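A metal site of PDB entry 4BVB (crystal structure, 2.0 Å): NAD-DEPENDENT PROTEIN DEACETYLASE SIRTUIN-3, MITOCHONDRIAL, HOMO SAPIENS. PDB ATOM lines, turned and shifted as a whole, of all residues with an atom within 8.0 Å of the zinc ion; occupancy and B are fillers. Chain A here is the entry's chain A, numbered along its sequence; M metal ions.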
ATOM      1  N   THR A 140      14.346  24.304 -15.844  1.00  0.00           N
ATOM      2  CA  THR A 140      15.703  24.614 -15.362  1.00  0.00           C
ATOM      3  C   THR A 140      15.803  26.008 -14.772  1.00  0.00           C
ATOM      4  O   THR A 140      15.278  26.969 -15.343  1.00  0.00           O
ATOM      5  CB  THR A 140      16.734  24.489 -16.520  1.00  0.00           C
ATOM      6  OG1 THR A 140      16.519  23.232 -17.153  1.00  0.00           O
ATOM      7  CG2 THR A 140      18.198  24.609 -16.018  1.00  0.00           C
ATOM      8  N   CYS A 141      16.493  26.147 -13.620  1.00  0.00           N
ATOM      9  CA  CYS A 141      16.808  27.465 -13.124  1.00  0.00           C
ATOM     10  C   CYS A 141      17.632  28.248 -14.165  1.00  0.00           C
ATOM     11  O   CYS A 141      18.667  27.766 -14.598  1.00  0.00           O
ATOM     12  CB  CYS A 141      17.583  27.416 -11.809  1.00  0.00           C
ATOM     13  SG  CYS A 141      17.756  29.104 -11.254  1.00  0.00           S
ATOM     14  N   THR A 142      17.181  29.442 -14.564  1.00  0.00           N
ATOM     15  CA  THR A 142      17.962  30.160 -15.584  1.00  0.00           C
ATOM     16  C   THR A 142      19.260  30.775 -14.978  1.00  0.00           C
ATOM     17  O   THR A 142      20.082  31.242 -15.750  1.00  0.00           O
ATOM     18  CB  THR A 142      17.180  31.339 -16.172  1.00  0.00           C
ATOM     19  OG1 THR A 142      16.876  32.256 -15.103  1.00  0.00           O
ATOM     20  CG2 THR A 142      15.847  30.877 -16.916  1.00  0.00           C
ATOM     21  N   VAL A 143      19.369  30.833 -13.648  1.00  0.00           N
ATOM     22  CA  VAL A 143      20.550  31.375 -12.963  1.00  0.00           C
ATOM     23  C   VAL A 143      21.525  30.240 -12.552  1.00  0.00           C
ATOM     24  O   VAL A 143      22.661  30.215 -13.064  1.00  0.00           O
ATOM     25  CB  VAL A 143      20.214  32.227 -11.702  1.00  0.00           C
ATOM     26  CG1 VAL A 143      21.509  32.748 -11.061  1.00  0.00           C
ATOM     27  CG2 VAL A 143      19.287  33.401 -12.006  1.00  0.00           C
ATOM     28  N   CYS A 144      21.101  29.314 -11.676  1.00  0.00           N
ATOM     29  CA  CYS A 144      22.020  28.256 -11.209  1.00  0.00           C
ATOM     30  C   CYS A 144      22.061  26.998 -12.045  1.00  0.00           C
ATOM     31  O   CYS A 144      22.812  26.094 -11.725  1.00  0.00           O
ATOM     32  CB  CYS A 144      21.818  27.920  -9.735  1.00  0.00           C
ATOM     33  SG  CYS A 144      20.299  26.954  -9.312  1.00  0.00           S
ATOM     34  N   GLN A 145      21.256  26.917 -13.112  1.00  0.00           N
ATOM     35  CA  GLN A 145      21.081  25.698 -13.927  1.00  0.00           C
ATOM     36  C   GLN A 145      20.537  24.452 -13.204  1.00  0.00           C
ATOM     37  O   GLN A 145      20.516  23.360 -13.778  1.00  0.00           O
ATOM     38  CB  GLN A 145      22.351  25.292 -14.697  1.00  0.00           C
ATOM     39  CG  GLN A 145      23.049  26.409 -15.462  1.00  0.00           C
ATOM     40  CD  GLN A 145      22.076  27.236 -16.267  1.00  0.00           C
ATOM     41  OE1 GLN A 145      21.368  26.729 -17.150  1.00  0.00           O
ATOM     42  NE2 GLN A 145      22.020  28.539 -15.963  1.00  0.00           N
ATOM     43  N   ARG A 146      20.039  24.585 -11.995  1.00  0.00           N
ATOM     44  CA  ARG A 146      19.397  23.416 -11.306  1.00  0.00           C
ATOM     45  C   ARG A 146      18.165  22.918 -12.107  1.00  0.00           C
ATOM     46  O   ARG A 146      17.258  23.707 -12.379  1.00  0.00           O
ATOM     47  CB  ARG A 146      18.985  23.833  -9.872  1.00  0.00           C
ATOM     48  CG  ARG A 146      18.194  22.773  -9.080  1.00  0.00           C
ATOM     49  CD  ARG A 146      18.146  23.044  -7.544  1.00  0.00           C
ATOM     50  NE  ARG A 146      17.323  22.035  -6.874  1.00  0.00           N
ATOM     51  CZ  ARG A 146      17.708  20.759  -6.702  1.00  0.00           C
ATOM     52  NH1 ARG A 146      18.917  20.411  -7.127  1.00  0.00           N
ATOM     53  NH2 ARG A 146      16.890  19.822  -6.124  1.00  0.00           N
ATOM     54  N   PRO A 147      18.139  21.618 -12.495  1.00  0.00           N
ATOM     55  CA  PRO A 147      16.935  21.058 -13.115  1.00  0.00           C
ATOM     56  C   PRO A 147      15.798  20.807 -12.113  1.00  0.00           C
ATOM     57  O   PRO A 147      16.025  20.682 -10.917  1.00  0.00           O
ATOM     58  CB  PRO A 147      17.420  19.745 -13.766  1.00  0.00           C
ATOM     59  CG  PRO A 147      18.944  19.826 -13.787  1.00  0.00           C
ATOM     60  CD  PRO A 147      19.252  20.649 -12.535  1.00  0.00           C
ATOM     61  N   PHE A 148      14.575  20.790 -12.629  1.00  0.00           N
ATOM     62  CA  PHE A 148      13.424  20.453 -11.830  1.00  0.00           C
ATOM     63  C   PHE A 148      12.488  19.657 -12.709  1.00  0.00           C
ATOM     64  O   PHE A 148      12.475  19.836 -13.938  1.00  0.00           O
ATOM     65  CB  PHE A 148      12.641  21.706 -11.399  1.00  0.00           C
ATOM     66  CG  PHE A 148      13.415  22.642 -10.534  1.00  0.00           C
ATOM     67  CD1 PHE A 148      13.386  22.521  -9.126  1.00  0.00           C
ATOM     68  CD2 PHE A 148      14.131  23.688 -11.115  1.00  0.00           C
ATOM     69  CE1 PHE A 148      14.114  23.398  -8.340  1.00  0.00           C
ATOM     70  CE2 PHE A 148      14.833  24.584 -10.310  1.00  0.00           C
ATOM     71  CZ  PHE A 148      14.839  24.449  -8.934  1.00  0.00           C
ATOM     72  N   ARG A 164      10.080  30.554  -9.161  1.00  0.00           N
ATOM     73  CA  ARG A 164      11.420  30.905  -8.680  1.00  0.00           C
ATOM     74  C   ARG A 164      12.179  29.697  -8.088  1.00  0.00           C
ATOM     75  O   ARG A 164      11.574  28.756  -7.586  1.00  0.00           O
ATOM     76  CB  ARG A 164      11.362  32.023  -7.649  1.00  0.00           C
ATOM     77  CG  ARG A 164      10.645  33.210  -8.208  1.00  0.00           C
ATOM     78  CD  ARG A 164      11.348  34.451  -7.790  1.00  0.00           C
ATOM     79  NE  ARG A 164      11.083  35.511  -8.754  1.00  0.00           N
ATOM     80  CZ  ARG A 164      12.034  36.140  -9.423  1.00  0.00           C
ATOM     81  NH1 ARG A 164      13.320  35.788  -9.256  1.00  0.00           N
ATOM     82  NH2 ARG A 164      11.685  37.106 -10.274  1.00  0.00           N
ATOM     83  N   CYS A 165      13.497  29.713  -8.245  1.00  0.00           N
ATOM     84  CA  CYS A 165      14.322  28.612  -7.844  1.00  0.00           C
ATOM     85  C   CYS A 165      14.461  28.631  -6.331  1.00  0.00           C
ATOM     86  O   CYS A 165      14.974  29.599  -5.781  1.00  0.00           O
ATOM     87  CB  CYS A 165      15.692  28.764  -8.459  1.00  0.00           C
ATOM     88  SG  CYS A 165      16.903  27.518  -7.949  1.00  0.00           S
ATOM     89  N   PRO A 166      14.055  27.521  -5.659  1.00  0.00           N
ATOM     90  CA  PRO A 166      14.129  27.575  -4.203  1.00  0.00           C
ATOM     91  C   PRO A 166      15.584  27.557  -3.669  1.00  0.00           C
ATOM     92  O   PRO A 166      15.780  27.808  -2.499  1.00  0.00           O
ATOM     93  CB  PRO A 166      13.328  26.352  -3.759  1.00  0.00           C
ATOM     94  CG  PRO A 166      13.426  25.382  -4.905  1.00  0.00           C
ATOM     95  CD  PRO A 166      13.665  26.171  -6.164  1.00  0.00           C
ATOM     96  N   VAL A 167      16.585  27.314  -4.520  1.00  0.00           N
ATOM     97  CA  VAL A 167      17.990  27.359  -4.109  1.00  0.00           C
ATOM     98  C   VAL A 167      18.549  28.776  -4.207  1.00  0.00           C
ATOM     99  O   VAL A 167      19.069  29.315  -3.230  1.00  0.00           O
ATOM    100  CB  VAL A 167      18.881  26.381  -4.908  1.00  0.00           C
ATOM    101  CG1 VAL A 167      20.346  26.733  -4.782  1.00  0.00           C
ATOM    102  CG2 VAL A 167      18.618  24.945  -4.462  1.00  0.00           C
ATOM    103  N   CYS A 168      18.465  29.356  -5.401  1.00  0.00           N
ATOM    104  CA  CYS A 168      19.038  30.676  -5.638  1.00  0.00           C
ATOM    105  C   CYS A 168      18.004  31.814  -5.879  1.00  0.00           C
ATOM    106  O   CYS A 168      18.403  32.941  -6.081  1.00  0.00           O
ATOM    107  CB  CYS A 168      20.031  30.583  -6.802  1.00  0.00           C
ATOM    108  SG  CYS A 168      19.270  30.611  -8.457  1.00  0.00           S
ATOM    109  N   THR A 169      16.714  31.501  -5.853  1.00  0.00           N
ATOM    110  CA  THR A 169      15.587  32.408  -6.263  1.00  0.00           C
ATOM    111  C   THR A 169      15.597  32.877  -7.743  1.00  0.00           C
ATOM    112  O   THR A 169      14.759  33.678  -8.118  1.00  0.00           O
ATOM    113  CB  THR A 169      15.336  33.600  -5.282  1.00  0.00           C
ATOM    114  OG1 THR A 169      16.238  34.682  -5.550  1.00  0.00           O
ATOM    115  CG2 THR A 169      15.495  33.185  -3.784  1.00  0.00           C
ATOM    116  N   GLY A 170      16.514  32.380  -8.595  1.00  0.00           N
ATOM    117  CA  GLY A 170      16.453  32.700 -10.052  1.00  0.00           C
ATOM    118  C   GLY A 170      15.122  32.233 -10.696  1.00  0.00           C
ATOM    119  O   GLY A 170      14.445  31.340 -10.157  1.00  0.00           O
ATOM    120  N   VAL A 171      14.723  32.826 -11.832  1.00  0.00           N
ATOM    121  CA  VAL A 171      13.450  32.443 -12.474  1.00  0.00           C
ATOM    122  C   VAL A 171      13.651  31.051 -13.081  1.00  0.00           C
ATOM    123  O   VAL A 171      14.656  30.797 -13.735  1.00  0.00           O
ATOM    124  CB  VAL A 171      12.999  33.501 -13.546  1.00  0.00           C
ATOM    125  CG1 VAL A 171      11.815  33.004 -14.366  1.00  0.00           C
ATOM    126  CG2 VAL A 171      12.657  34.793 -12.792  1.00  0.00           C
ATOM    127  N   VAL A 172      12.716  30.138 -12.795  1.00  0.00           N
ATOM    128  CA  VAL A 172      12.759  28.794 -13.405  1.00  0.00           C
ATOM    129  C   VAL A 172      12.016  28.807 -14.755  1.00  0.00           C
ATOM    130  O   VAL A 172      10.913  29.361 -14.822  1.00  0.00           O
ATOM    131  CB  VAL A 172      12.213  27.718 -12.431  1.00  0.00           C
ATOM    132  CG1 VAL A 172      12.271  26.328 -13.049  1.00  0.00           C
ATOM    133  CG2 VAL A 172      12.986  27.755 -11.116  1.00  0.00           C
HETATM  134 ZN    ZN M   1      18.618  28.497  -9.056  1.00  0.00          ZN
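The backbone carbonyl oxygen (O) of Gly 170 sits at hydrogen-bond distance from the backbone NH (N) of Cys 165 (2.7 Å). SG of Cys 165 sits close to N of Val 167 (3.4 Å). SG of Cys 168 sits close to N of Gly 170 (3.3 Å). SG of Cys 144 lies close to N of Arg 146. N of Cys 141 sits at hydrogen-bond distance from O of Arg 146 (2.8 Å). The side-chain sulfur (SG) of Cys 141 sits close to the backbone NH (N) of Val 143, 3.4 Å away.
The nearest printed residue that does not touch the zinc ion is Gly 170 (4.4 Å).
The zinc ion is bound by the side-chain sulfur of Cys 165 (2.3 Å), the side-chain sulfur of Cys 168 (2.3 Å), the side-chain sulfur of Cys 144 (2.3 Å) and the side-chain sulfur of Cys 141 (2.4 Å).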
